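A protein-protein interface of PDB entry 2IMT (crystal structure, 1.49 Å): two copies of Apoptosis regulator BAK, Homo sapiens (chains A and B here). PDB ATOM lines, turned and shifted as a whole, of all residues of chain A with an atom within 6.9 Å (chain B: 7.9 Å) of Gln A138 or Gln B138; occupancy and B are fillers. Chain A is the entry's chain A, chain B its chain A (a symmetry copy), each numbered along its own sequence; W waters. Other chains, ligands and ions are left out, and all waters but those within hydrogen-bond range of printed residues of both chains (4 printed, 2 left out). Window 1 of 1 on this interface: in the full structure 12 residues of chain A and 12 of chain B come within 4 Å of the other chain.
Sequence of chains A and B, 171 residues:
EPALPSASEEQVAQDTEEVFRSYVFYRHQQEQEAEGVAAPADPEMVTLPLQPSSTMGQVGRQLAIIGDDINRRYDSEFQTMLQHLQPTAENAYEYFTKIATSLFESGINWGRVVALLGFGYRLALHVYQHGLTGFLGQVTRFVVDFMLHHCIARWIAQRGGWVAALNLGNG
NH1 of Arg A141 is in hydrogen-bond range of O of Gly A137. The side-chain amide oxygen (OE1) of Gln A138 is in hydrogen-bond range of the guanidinium group (NH2) of Arg A141 (2.8 Å). The backbone carbonyl oxygen (O) of Gly B137 lies within hydrogen-bond range of the guanidinium group (NH1) of Arg B141, 3.3 Å away. OE1 of Gln B138 sits at hydrogen-bond distance from NH2 of Arg B141 (2.8 Å).
O of Gly B134 sits at hydrogen-bond distance from N of Glu A90, 3.1 Å away. The side-chain carboxylate of Glu A90 is in salt-bridge range of the guanidinium group of Arg B141 (2.9 Å). The backbone NH (N) of Glu B90 sits at hydrogen-bond distance from the backbone carbonyl oxygen (O) of Gly A134 (3.1 Å). NE2 of Gln A138 lies close to NE2 of Gln B138 (3.4 Å). The side-chain carboxylate (OE1) of Glu B90 lies within salt-bridge range of the guanidinium group (NH1) of Arg A141 (2.9 Å).
Of the 13 printed residues of chain A, 9 touch a printed residue of chain B. Printed residues of chain A that touch a printed residue of chain B: Ala A89, Glu A90, Tyr A93, Gly A134, Phe A135, Gly A137, Gln A138, Arg A141 and Phe A142. Hydrophobic or aromatic side chains of chain A within 4 Å of the printed part of chain B: Ala A89, Tyr A93, Phe A135 and Phe A142. Along chain A the printed residues that touch a printed residue of chain B span positions 89 to 142. Hydrophobic or aromatic side chains of chain B that line the printed part of chain A: Ala B89, Tyr B93, Phe B135 and Phe B142.
Among the printed residues, merely in contact across the chains: Gln A138 with Phe B142, Phe A142 with Gln B138, Tyr A93 with Arg B141, Arg A141 with Tyr B93, Gly A137 with Glu B90, Glu A90 with Gly B137, Ala A89 with Phe B135, Phe A135 with Ala B89, Gly A134 with Ala B89, Ala A89 with Gly B134, Arg A141 with Ala B89 and Ala A89 with Arg B141.
Water W4 bridges OE2 of Glu A90 (2.7 Å) and NH1 of Arg B141 (3.4 Å). Water W3 lies within hydrogen-bond range of the side-chain carboxylate (OE2) of Glu B90 (2.7 Å) and the guanidinium group (NH1) of Arg A141 (3.4 Å). Water W2 bridges NE2 of Gln A138 (2.9 Å) and NE2 of Gln B138 (3.5 Å). Water W1 bridges the side-chain amide nitrogen of Gln B138 (2.9 Å) and the side-chain amide nitrogen of Gln A138 (3.5 Å).
Ala A89 touches Gly B134, and with the chains exchanged Gly A134 touches Ala B89. Ala A89 touches Arg B141, and with the chains exchanged Arg A141 touches Ala B89. Glu A90 touches Gly B134, and with the chains exchanged Gly A134 touches Glu B90. Glu A90 touches Arg B141, and with the chains exchanged Arg A141 touches Glu B90. 13 positions are printed for both chains. Of the 17 pairs that touch across the chains among the printed residues, 17 have their exchanged pair printed and touching as well.
Of the printed residues of chain B, Tyr A93 touches Arg B141 (3.4 Å). Of the printed residues of chain B, Gly A134 touches Ala B89 (3.7 Å) and Glu B90 (3.1 Å). Printed residues of chain B within 4 Å of Phe A135: Ala B89. Gly A137 touches just one residue of chain B: Glu B90 (3.5 Å). Gln A138 touches just these residues of chain B: Gln B138 (3.4 Å) and Phe B142 (3.4 Å). Of the printed residues of chain A, Tyr B93 touches Arg A141 (3.4 Å). Gln B138 touches just these residues of chain A: Gln A138 and Phe A142. Printed residues of chain A within 4 Å of Phe B142: Gln A138 (3.4 Å). The nearest residue of chain B that does not touch Gln A138 is Glu B90 (4.03 Å). The nearest residue of chain A that does not touch Gln B138 is Glu A90 (4.03 Å).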
ATOM      1  N   ALA A  89      31.125 -13.811 -16.272  1.00  0.00           N
ATOM      2  CA  ALA A  89      30.093 -13.334 -15.426  1.00  0.00           C
ATOM      3  C   ALA A  89      30.017 -14.249 -14.205  1.00  0.00           C
ATOM      4  O   ALA A  89      29.834 -13.778 -13.069  1.00  0.00           O
ATOM      5  CB  ALA A  89      28.809 -13.238 -16.201  1.00  0.00           C
ATOM      6  N   GLU A  90      30.149 -15.581 -14.432  1.00  0.00           N
ATOM      7  CA  GLU A  90      30.005 -16.512 -13.384  1.00  0.00           C
ATOM      8  C   GLU A  90      31.123 -16.415 -12.356  1.00  0.00           C
ATOM      9  O   GLU A  90      30.839 -16.463 -11.176  1.00  0.00           O
ATOM     10  CB  GLU A  90      29.868 -17.948 -13.941  1.00  0.00           C
ATOM     11  CG  GLU A  90      29.383 -18.918 -12.859  1.00  0.00           C
ATOM     12  CD  GLU A  90      28.034 -18.570 -12.264  1.00  0.00           C
ATOM     13  OE1 GLU A  90      27.289 -17.734 -12.810  1.00  0.00           O
ATOM     14  OE2 GLU A  90      27.738 -19.119 -11.204  1.00  0.00           O
ATOM     15  N   TYR A  93      30.669 -13.183 -10.364  1.00  0.00           N
ATOM     16  CA  TYR A  93      29.635 -13.301  -9.371  1.00  0.00           C
ATOM     17  C   TYR A  93      30.058 -14.144  -8.217  1.00  0.00           C
ATOM     18  O   TYR A  93      29.864 -13.760  -7.062  1.00  0.00           O
ATOM     19  CB  TYR A  93      28.434 -13.912  -9.957  1.00  0.00           C
ATOM     20  CG  TYR A  93      27.391 -14.270  -8.933  1.00  0.00           C
ATOM     21  CD1 TYR A  93      26.660 -13.262  -8.342  1.00  0.00           C
ATOM     22  CD2 TYR A  93      27.193 -15.590  -8.519  1.00  0.00           C
ATOM     23  CE1 TYR A  93      25.717 -13.518  -7.459  1.00  0.00           C
ATOM     24  CE2 TYR A  93      26.223 -15.871  -7.567  1.00  0.00           C
ATOM     25  CZ  TYR A  93      25.543 -14.783  -7.017  1.00  0.00           C
ATOM     26  OH  TYR A  93      24.542 -14.852  -6.077  1.00  0.00           O
ATOM     27  N   GLY A 134      31.052  -3.881 -20.976  1.00  0.00           N
ATOM     28  CA  GLY A 134      29.589  -3.892 -20.776  1.00  0.00           C
ATOM     29  C   GLY A 134      29.142  -4.548 -19.502  1.00  0.00           C
ATOM     30  O   GLY A 134      28.022  -5.026 -19.385  1.00  0.00           O
ATOM     31  N   PHE A 135      30.054  -4.623 -18.527  1.00  0.00           N
ATOM     32  CA  PHE A 135      29.816  -5.391 -17.271  1.00  0.00           C
ATOM     33  C   PHE A 135      29.704  -4.474 -16.034  1.00  0.00           C
ATOM     34  O   PHE A 135      29.493  -4.964 -14.913  1.00  0.00           O
ATOM     35  CB  PHE A 135      30.918  -6.383 -17.040  1.00  0.00           C
ATOM     36  CG  PHE A 135      30.532  -7.525 -16.193  1.00  0.00           C
ATOM     37  CD1 PHE A 135      29.731  -8.539 -16.725  1.00  0.00           C
ATOM     38  CD2 PHE A 135      30.941  -7.661 -14.884  1.00  0.00           C
ATOM     39  CE1 PHE A 135      29.326  -9.598 -15.903  1.00  0.00           C
ATOM     40  CE2 PHE A 135      30.502  -8.739 -14.103  1.00  0.00           C
ATOM     41  CZ  PHE A 135      29.710  -9.676 -14.646  1.00  0.00           C
ATOM     42  N   LEU A 136      29.926  -3.177 -16.226  1.00  0.00           N
ATOM     43  CA  LEU A 136      29.819  -2.258 -15.072  1.00  0.00           C
ATOM     44  C   LEU A 136      28.414  -2.232 -14.472  1.00  0.00           C
ATOM     45  O   LEU A 136      28.240  -2.216 -13.224  1.00  0.00           O
ATOM     46  CB  LEU A 136      30.334  -0.866 -15.423  1.00  0.00           C
ATOM     47  CG  LEU A 136      30.372   0.206 -14.317  1.00  0.00           C
ATOM     48  CD1 LEU A 136      31.204  -0.224 -13.134  1.00  0.00           C
ATOM     49  CD2 LEU A 136      30.910   1.500 -15.029  1.00  0.00           C
ATOM     50  N   GLY A 137      27.418  -2.178 -15.333  1.00  0.00           N
ATOM     51  CA  GLY A 137      26.052  -2.292 -14.859  1.00  0.00           C
ATOM     52  C   GLY A 137      25.763  -3.567 -14.121  1.00  0.00           C
ATOM     53  O   GLY A 137      25.045  -3.547 -13.114  1.00  0.00           O
ATOM     54  N   GLN A 138      26.377  -4.675 -14.519  1.00  0.00           N
ATOM     55  CA  GLN A 138      26.241  -5.955 -13.820  1.00  0.00           C
ATOM     56  C   GLN A 138      26.868  -5.908 -12.402  1.00  0.00           C
ATOM     57  O   GLN A 138      26.293  -6.427 -11.449  1.00  0.00           O
ATOM     58  CB  GLN A 138      26.768  -7.137 -14.633  1.00  0.00           C
ATOM     59  CG  GLN A 138      26.309  -8.426 -14.003  1.00  0.00           C
ATOM     60  CD  GLN A 138      24.768  -8.557 -13.880  1.00  0.00           C
ATOM     61  OE1 GLN A 138      24.049  -8.418 -14.872  1.00  0.00           O
ATOM     62  NE2 GLN A 138      24.264  -8.659 -12.620  1.00  0.00           N
ATOM     63  N   VAL A 139      28.059  -5.294 -12.271  1.00  0.00           N
ATOM     64  CA  VAL A 139      28.605  -5.188 -10.979  1.00  0.00           C
ATOM     65  C   VAL A 139      27.712  -4.296 -10.134  1.00  0.00           C
ATOM     66  O   VAL A 139      27.547  -4.546  -8.959  1.00  0.00           O
ATOM     67  CB  VAL A 139      30.029  -4.598 -11.061  1.00  0.00           C
ATOM     68  CG1 VAL A 139      30.520  -4.317  -9.610  1.00  0.00           C
ATOM     69  CG2 VAL A 139      30.944  -5.560 -11.756  1.00  0.00           C
ATOM     70  N   THR A 140      27.148  -3.252 -10.710  1.00  0.00           N
ATOM     71  CA  THR A 140      26.291  -2.323  -9.922  1.00  0.00           C
ATOM     72  C   THR A 140      25.109  -3.174  -9.371  1.00  0.00           C
ATOM     73  O   THR A 140      24.731  -3.070  -8.222  1.00  0.00           O
ATOM     74  CB  THR A 140      25.775  -1.207 -10.823  1.00  0.00           C
ATOM     75  OG1 THR A 140      26.880  -0.386 -11.358  1.00  0.00           O
ATOM     76  CG2 THR A 140      24.778  -0.302 -10.184  1.00  0.00           C
ATOM     77  N   ARG A 141      24.507  -3.971 -10.237  1.00  0.00           N
ATOM     78  CA  ARG A 141      23.426  -4.908  -9.868  1.00  0.00           C
ATOM     79  C   ARG A 141      23.833  -5.896  -8.772  1.00  0.00           C
ATOM     80  O   ARG A 141      23.000  -6.187  -7.858  1.00  0.00           O
ATOM     81  CB  ARG A 141      22.878  -5.596 -11.093  1.00  0.00           C
ATOM     82  CG  ARG A 141      22.076  -4.683 -11.916  1.00  0.00           C
ATOM     83  CD  ARG A 141      21.386  -5.382 -13.129  1.00  0.00           C
ATOM     84  NE  ARG A 141      22.236  -5.991 -14.123  1.00  0.00           N
ATOM     85  CZ  ARG A 141      22.803  -5.329 -15.140  1.00  0.00           C
ATOM     86  NH1 ARG A 141      22.670  -4.054 -15.291  1.00  0.00           N
ATOM     87  NH2 ARG A 141      23.539  -5.950 -15.993  1.00  0.00           N
ATOM     88  N   PHE A 142      25.072  -6.392  -8.811  1.00  0.00           N
ATOM     89  CA  PHE A 142      25.669  -7.292  -7.783  1.00  0.00           C
ATOM     90  C   PHE A 142      25.579  -6.504  -6.421  1.00  0.00           C
ATOM     91  O   PHE A 142      25.139  -7.004  -5.446  1.00  0.00           O
ATOM     92  CB  PHE A 142      27.119  -7.652  -8.049  1.00  0.00           C
ATOM     93  CG  PHE A 142      27.315  -8.738  -9.137  1.00  0.00           C
ATOM     94  CD1 PHE A 142      26.282  -9.382  -9.744  1.00  0.00           C
ATOM     95  CD2 PHE A 142      28.564  -8.972  -9.598  1.00  0.00           C
ATOM     96  CE1 PHE A 142      26.576 -10.333 -10.790  1.00  0.00           C
ATOM     97  CE2 PHE A 142      28.816  -9.930 -10.623  1.00  0.00           C
ATOM     98  CZ  PHE A 142      27.872 -10.581 -11.151  1.00  0.00           C
ATOM     99  N   VAL A 143      26.028  -5.304  -6.455  1.00  0.00           N
ATOM    100  CA  VAL A 143      26.064  -4.466  -5.241  1.00  0.00           C
ATOM    101  C   VAL A 143      24.706  -4.142  -4.702  1.00  0.00           C
ATOM    102  O   VAL A 143      24.476  -4.380  -3.504  1.00  0.00           O
ATOM    103  CB  VAL A 143      26.921  -3.184  -5.461  1.00  0.00           C
ATOM    104  CG1 VAL A 143      26.838  -2.282  -4.229  1.00  0.00           C
ATOM    105  CG2 VAL A 143      28.379  -3.597  -5.791  1.00  0.00           C
ATOM    106  N   PHE B  20      14.443 -23.392 -12.877  1.00  0.00           N
ATOM    107  CA  PHE B  20      15.043 -22.891 -14.104  1.00  0.00           C
ATOM    108  C   PHE B  20      16.206 -23.735 -14.664  1.00  0.00           C
ATOM    109  O   PHE B  20      16.154 -24.075 -15.842  1.00  0.00           O
ATOM    110  CB  PHE B  20      15.445 -21.435 -14.013  1.00  0.00           C
ATOM    111  CG  PHE B  20      16.006 -20.880 -15.303  1.00  0.00           C
ATOM    112  CD1 PHE B  20      15.157 -20.623 -16.336  1.00  0.00           C
ATOM    113  CD2 PHE B  20      17.356 -20.628 -15.485  1.00  0.00           C
ATOM    114  CE1 PHE B  20      15.589 -20.129 -17.549  1.00  0.00           C
ATOM    115  CE2 PHE B  20      17.818 -20.082 -16.693  1.00  0.00           C
ATOM    116  CZ  PHE B  20      16.942 -19.849 -17.745  1.00  0.00           C
ATOM    117  N   THR B  88      26.722  -8.529 -24.548  1.00  0.00           N
ATOM    118  CA  THR B  88      27.271  -7.998 -23.326  1.00  0.00           C
ATOM    119  C   THR B  88      26.179  -8.214 -22.311  1.00  0.00           C
ATOM    120  O   THR B  88      24.960  -8.310 -22.661  1.00  0.00           O
ATOM    121  CB  THR B  88      27.579  -6.478 -23.355  1.00  0.00           C
ATOM    122  OG1 THR B  88      26.359  -5.747 -23.558  1.00  0.00           O
ATOM    123  CG2 THR B  88      28.408  -6.103 -24.517  1.00  0.00           C
ATOM    124  N   ALA B  89      26.665  -8.173 -21.100  1.00  0.00           N
ATOM    125  CA  ALA B  89      25.874  -8.374 -19.941  1.00  0.00           C
ATOM    126  C   ALA B  89      24.803  -7.285 -19.899  1.00  0.00           C
ATOM    127  O   ALA B  89      23.639  -7.552 -19.553  1.00  0.00           O
ATOM    128  CB  ALA B  89      26.759  -8.409 -18.727  1.00  0.00           C
ATOM    129  N   GLU B  90      25.193  -6.032 -20.247  1.00  0.00           N
ATOM    130  CA  GLU B  90      24.302  -4.945 -20.155  1.00  0.00           C
ATOM    131  C   GLU B  90      23.160  -5.038 -21.156  1.00  0.00           C
ATOM    132  O   GLU B  90      22.033  -4.776 -20.783  1.00  0.00           O
ATOM    133  CB  GLU B  90      25.060  -3.602 -20.281  1.00  0.00           C
ATOM    134  CG  GLU B  90      24.176  -2.425 -19.857  1.00  0.00           C
ATOM    135  CD  GLU B  90      23.683  -2.495 -18.426  1.00  0.00           C
ATOM    136  OE1 GLU B  90      24.186  -3.294 -17.613  1.00  0.00           O
ATOM    137  OE2 GLU B  90      22.745  -1.759 -18.127  1.00  0.00           O
ATOM    138  N   ALA B  92      22.170  -7.766 -22.572  1.00  0.00           N
ATOM    139  CA  ALA B  92      21.383  -8.940 -22.113  1.00  0.00           C
ATOM    140  C   ALA B  92      20.346  -8.561 -21.057  1.00  0.00           C
ATOM    141  O   ALA B  92      19.161  -8.943 -21.126  1.00  0.00           O
ATOM    142  CB  ALA B  92      22.260 -10.007 -21.614  1.00  0.00           C
ATOM    143  N   TYR B  93      20.807  -7.845 -20.059  1.00  0.00           N
ATOM    144  CA  TYR B  93      19.953  -7.442 -18.974  1.00  0.00           C
ATOM    145  C   TYR B  93      18.886  -6.501 -19.419  1.00  0.00           C
ATOM    146  O   TYR B  93      17.715  -6.679 -19.073  1.00  0.00           O
ATOM    147  CB  TYR B  93      20.739  -6.768 -17.931  1.00  0.00           C
ATOM    148  CG  TYR B  93      19.887  -6.124 -16.871  1.00  0.00           C
ATOM    149  CD1 TYR B  93      19.245  -6.924 -15.951  1.00  0.00           C
ATOM    150  CD2 TYR B  93      19.679  -4.743 -16.838  1.00  0.00           C
ATOM    151  CE1 TYR B  93      18.509  -6.414 -14.985  1.00  0.00           C
ATOM    152  CE2 TYR B  93      18.881  -4.194 -15.843  1.00  0.00           C
ATOM    153  CZ  TYR B  93      18.262  -5.086 -14.965  1.00  0.00           C
ATOM    154  OH  TYR B  93      17.450  -4.742 -13.910  1.00  0.00           O
ATOM    155  N   GLU B  94      19.231  -5.485 -20.208  1.00  0.00           N
ATOM    156  CA  GLU B  94      18.257  -4.568 -20.741  1.00  0.00           C
ATOM    157  C   GLU B  94      17.152  -5.264 -21.555  1.00  0.00           C
ATOM    158  O   GLU B  94      15.991  -4.972 -21.397  1.00  0.00           O
ATOM    159  CB  GLU B  94      18.955  -3.475 -21.599  1.00  0.00           C
ATOM    160  CG  GLU B  94      19.754  -2.500 -20.717  1.00  0.00           C
ATOM    161  CD  GLU B  94      20.428  -1.428 -21.566  1.00  0.00           C
ATOM    162  OE1 GLU B  94      19.873  -0.334 -21.615  1.00  0.00           O
ATOM    163  OE2 GLU B  94      21.457  -1.686 -22.211  1.00  0.00           O
ATOM    164  N   PHE B  96      16.383  -8.515 -21.415  1.00  0.00           N
ATOM    165  CA  PHE B  96      15.679  -9.428 -20.557  1.00  0.00           C
ATOM    166  C   PHE B  96      14.561  -8.693 -19.814  1.00  0.00           C
ATOM    167  O   PHE B  96      13.434  -9.158 -19.707  1.00  0.00           O
ATOM    168  CB  PHE B  96      16.627 -10.042 -19.532  1.00  0.00           C
ATOM    169  CG  PHE B  96      15.909 -10.868 -18.535  1.00  0.00           C
ATOM    170  CD1 PHE B  96      15.573 -12.193 -18.773  1.00  0.00           C
ATOM    171  CD2 PHE B  96      15.555 -10.324 -17.346  1.00  0.00           C
ATOM    172  CE1 PHE B  96      14.790 -12.921 -17.772  1.00  0.00           C
ATOM    173  CE2 PHE B  96      14.783 -11.012 -16.357  1.00  0.00           C
ATOM    174  CZ  PHE B  96      14.426 -12.342 -16.589  1.00  0.00           C
ATOM    175  N   LEU B 123      17.429 -16.564 -24.517  1.00  0.00           N
ATOM    176  CA  LEU B 123      18.395 -15.533 -24.264  1.00  0.00           C
ATOM    177  C   LEU B 123      19.778 -16.161 -23.972  1.00  0.00           C
ATOM    178  O   LEU B 123      20.768 -15.751 -24.618  1.00  0.00           O
ATOM    179  CB  LEU B 123      17.975 -14.624 -23.127  1.00  0.00           C
ATOM    180  CG  LEU B 123      19.092 -13.657 -22.630  1.00  0.00           C
ATOM    181  CD1 LEU B 123      19.503 -12.684 -23.663  1.00  0.00           C
ATOM    182  CD2 LEU B 123      18.616 -12.880 -21.434  1.00  0.00           C
ATOM    183  N   ALA B 124      19.826 -17.145 -23.077  1.00  0.00           N
ATOM    184  CA  ALA B 124      21.028 -17.803 -22.689  1.00  0.00           C
ATOM    185  C   ALA B 124      21.690 -18.493 -23.906  1.00  0.00           C
ATOM    186  O   ALA B 124      22.927 -18.373 -24.170  1.00  0.00           O
ATOM    187  CB  ALA B 124      20.779 -18.718 -21.550  1.00  0.00           C
ATOM    188  N   LEU B 132      29.384 -15.305 -25.709  1.00  0.00           N
ATOM    189  CA  LEU B 132      29.452 -14.934 -24.307  1.00  0.00           C
ATOM    190  C   LEU B 132      29.319 -16.231 -23.495  1.00  0.00           C
ATOM    191  O   LEU B 132      28.231 -16.757 -23.350  1.00  0.00           O
ATOM    192  CB  LEU B 132      28.309 -13.976 -23.983  1.00  0.00           C
ATOM    193  CG  LEU B 132      28.229 -13.429 -22.578  1.00  0.00           C
ATOM    194  CD1 LEU B 132      29.524 -12.557 -22.322  1.00  0.00           C
ATOM    195  CD2 LEU B 132      27.027 -12.541 -22.464  1.00  0.00           C
ATOM    196  N   GLY B 134      29.962 -18.589 -19.945  1.00  0.00           N
ATOM    197  CA  GLY B 134      29.920 -18.351 -18.488  1.00  0.00           C
ATOM    198  C   GLY B 134      28.801 -17.459 -18.038  1.00  0.00           C
ATOM    199  O   GLY B 134      28.868 -16.821 -16.996  1.00  0.00           O
ATOM    200  N   PHE B 135      27.754 -17.363 -18.866  1.00  0.00           N
ATOM    201  CA  PHE B 135      26.646 -16.392 -18.640  1.00  0.00           C
ATOM    202  C   PHE B 135      25.315 -17.090 -18.288  1.00  0.00           C
ATOM    203  O   PHE B 135      24.299 -16.414 -18.059  1.00  0.00           O
ATOM    204  CB  PHE B 135      26.437 -15.534 -19.854  1.00  0.00           C
ATOM    205  CG  PHE B 135      25.798 -14.237 -19.572  1.00  0.00           C
ATOM    206  CD1 PHE B 135      26.543 -13.215 -18.979  1.00  0.00           C
ATOM    207  CD2 PHE B 135      24.484 -13.965 -19.885  1.00  0.00           C
ATOM    208  CE1 PHE B 135      25.919 -12.000 -18.669  1.00  0.00           C
ATOM    209  CE2 PHE B 135      23.906 -12.733 -19.547  1.00  0.00           C
ATOM    210  CZ  PHE B 135      24.651 -11.788 -18.952  1.00  0.00           C
ATOM    211  N   LEU B 136      25.305 -18.420 -18.330  1.00  0.00           N
ATOM    212  CA  LEU B 136      24.055 -19.133 -17.990  1.00  0.00           C
ATOM    213  C   LEU B 136      23.607 -18.879 -16.552  1.00  0.00           C
ATOM    214  O   LEU B 136      22.394 -18.685 -16.273  1.00  0.00           O
ATOM    215  CB  LEU B 136      24.159 -20.619 -18.321  1.00  0.00           C
ATOM    216  CG  LEU B 136      22.919 -21.509 -18.105  1.00  0.00           C
ATOM    217  CD1 LEU B 136      21.725 -21.024 -18.888  1.00  0.00           C
ATOM    218  CD2 LEU B 136      23.389 -22.955 -18.502  1.00  0.00           C
ATOM    219  N   GLY B 137      24.553 -18.926 -15.635  1.00  0.00           N
ATOM    220  CA  GLY B 137      24.244 -18.558 -14.267  1.00  0.00           C
ATOM    221  C   GLY B 137      23.720 -17.160 -14.109  1.00  0.00           C
ATOM    222  O   GLY B 137      22.801 -16.933 -13.314  1.00  0.00           O
ATOM    223  N   GLN B 138      24.198 -16.217 -14.913  1.00  0.00           N
ATOM    224  CA  GLN B 138      23.697 -14.841 -14.910  1.00  0.00           C
ATOM    225  C   GLN B 138      22.228 -14.760 -15.402  1.00  0.00           C
ATOM    226  O   GLN B 138      21.419 -14.032 -14.832  1.00  0.00           O
ATOM    227  CB  GLN B 138      24.603 -13.875 -15.675  1.00  0.00           C
ATOM    228  CG  GLN B 138      24.204 -12.457 -15.361  1.00  0.00           C
ATOM    229  CD  GLN B 138      24.262 -12.101 -13.853  1.00  0.00           C
ATOM    230  OE1 GLN B 138      25.296 -12.288 -13.207  1.00  0.00           O
ATOM    231  NE2 GLN B 138      23.088 -11.746 -13.264  1.00  0.00           N
ATOM    232  N   VAL B 139      21.891 -15.503 -16.473  1.00  0.00           N
ATOM    233  CA  VAL B 139      20.546 -15.488 -16.886  1.00  0.00           C
ATOM    234  C   VAL B 139      19.687 -16.116 -15.802  1.00  0.00           C
ATOM    235  O   VAL B 139      18.580 -15.673 -15.578  1.00  0.00           O
ATOM    236  CB  VAL B 139      20.399 -16.272 -18.208  1.00  0.00           C
ATOM    237  CG1 VAL B 139      18.879 -16.397 -18.528  1.00  0.00           C
ATOM    238  CG2 VAL B 139      21.117 -15.557 -19.311  1.00  0.00           C
ATOM    239  N   THR B 140      20.172 -17.148 -15.139  1.00  0.00           N
ATOM    240  CA  THR B 140      19.360 -17.825 -14.090  1.00  0.00           C
ATOM    241  C   THR B 140      19.055 -16.749 -13.006  1.00  0.00           C
ATOM    242  O   THR B 140      17.950 -16.628 -12.521  1.00  0.00           O
ATOM    243  CB  THR B 140      20.150 -18.982 -13.491  1.00  0.00           C
ATOM    244  OG1 THR B 140      20.450 -20.016 -14.503  1.00  0.00           O
ATOM    245  CG2 THR B 140      19.502 -19.638 -12.321  1.00  0.00           C
ATOM    246  N   ARG B 141      20.080 -16.016 -12.605  1.00  0.00           N
ATOM    247  CA  ARG B 141      19.957 -14.897 -11.648  1.00  0.00           C
ATOM    248  C   ARG B 141      18.967 -13.820 -12.104  1.00  0.00           C
ATOM    249  O   ARG B 141      18.194 -13.287 -11.249  1.00  0.00           O
ATOM    250  CB  ARG B 141      21.314 -14.331 -11.314  1.00  0.00           C
ATOM    251  CG  ARG B 141      22.085 -15.240 -10.457  1.00  0.00           C
ATOM    252  CD  ARG B 141      23.448 -14.642  -9.983  1.00  0.00           C
ATOM    253  NE  ARG B 141      24.420 -14.308 -10.996  1.00  0.00           N
ATOM    254  CZ  ARG B 141      25.273 -15.186 -11.541  1.00  0.00           C
ATOM    255  NH1 ARG B 141      25.263 -16.439 -11.233  1.00  0.00           N
ATOM    256  NH2 ARG B 141      26.120 -14.804 -12.431  1.00  0.00           N
ATOM    257  N   PHE B 142      18.943 -13.508 -13.402  1.00  0.00           N
ATOM    258  CA  PHE B 142      17.990 -12.554 -14.037  1.00  0.00           C
ATOM    259  C   PHE B 142      16.551 -13.111 -13.717  1.00  0.00           C
ATOM    260  O   PHE B 142      15.704 -12.417 -13.276  1.00  0.00           O
ATOM    261  CB  PHE B 142      18.149 -12.437 -15.542  1.00  0.00           C
ATOM    262  CG  PHE B 142      19.348 -11.563 -15.989  1.00  0.00           C
ATOM    263  CD1 PHE B 142      20.141 -10.882 -15.118  1.00  0.00           C
ATOM    264  CD2 PHE B 142      19.702 -11.571 -17.293  1.00  0.00           C
ATOM    265  CE1 PHE B 142      21.269 -10.146 -15.638  1.00  0.00           C
ATOM    266  CE2 PHE B 142      20.815 -10.820 -17.771  1.00  0.00           C
ATOM    267  CZ  PHE B 142      21.523 -10.133 -16.982  1.00  0.00           C
ATOM    268  N   VAL B 143      16.375 -14.352 -13.983  1.00  0.00           N
ATOM    269  CA  VAL B 143      15.061 -14.998 -13.792  1.00  0.00           C
ATOM    270  C   VAL B 143      14.629 -15.050 -12.359  1.00  0.00           C
ATOM    271  O   VAL B 143      13.505 -14.607 -12.067  1.00  0.00           O
ATOM    272  CB  VAL B 143      15.015 -16.402 -14.464  1.00  0.00           C
ATOM    273  CG1 VAL B 143      13.688 -17.091 -14.144  1.00  0.00           C
ATOM    274  CG2 VAL B 143      15.243 -16.243 -15.989  1.00  0.00           C
ATOM    275  N   VAL B 144      15.477 -15.543 -11.485  1.00  0.00           N
ATOM    276  CA  VAL B 144      15.181 -15.698 -10.056  1.00  0.00           C
ATOM    277  C   VAL B 144      14.816 -14.368  -9.464  1.00  0.00           C
ATOM    278  O   VAL B 144      13.825 -14.200  -8.780  1.00  0.00           O
ATOM    279  CB  VAL B 144      16.364 -16.326  -9.290  1.00  0.00           C
ATOM    280  CG1 VAL B 144      16.132 -16.313  -7.753  1.00  0.00           C
ATOM    281  CG2 VAL B 144      16.738 -17.759  -9.766  1.00  0.00           C
ATOM    282  N   ASP B 145      15.612 -13.359  -9.784  1.00  0.00           N
ATOM    283  CA  ASP B 145      15.445 -12.043  -9.156  1.00  0.00           C
ATOM    284  C   ASP B 145      14.226 -11.291  -9.692  1.00  0.00           C
ATOM    285  O   ASP B 145      13.517 -10.612  -8.905  1.00  0.00           O
ATOM    286  CB  ASP B 145      16.724 -11.230  -9.280  1.00  0.00           C
ATOM    287  CG  ASP B 145      16.877 -10.209  -8.096  1.00  0.00           C
ATOM    288  OD1 ASP B 145      16.883 -10.671  -6.943  1.00  0.00           O
ATOM    289  OD2 ASP B 145      17.006  -9.048  -8.373  1.00  0.00           O
HETATM  290  O   HOH W   1      23.069 -11.081 -10.459  1.00  0.00           O
HETATM  291  O   HOH W   2      21.412  -8.890 -12.266  1.00  0.00           O
HETATM  292  O   HOH W   3      22.199  -0.765 -15.725  1.00  0.00           O
HETATM  293  O   HOH W   4      25.295 -19.662 -10.315  1.00  0.00           O
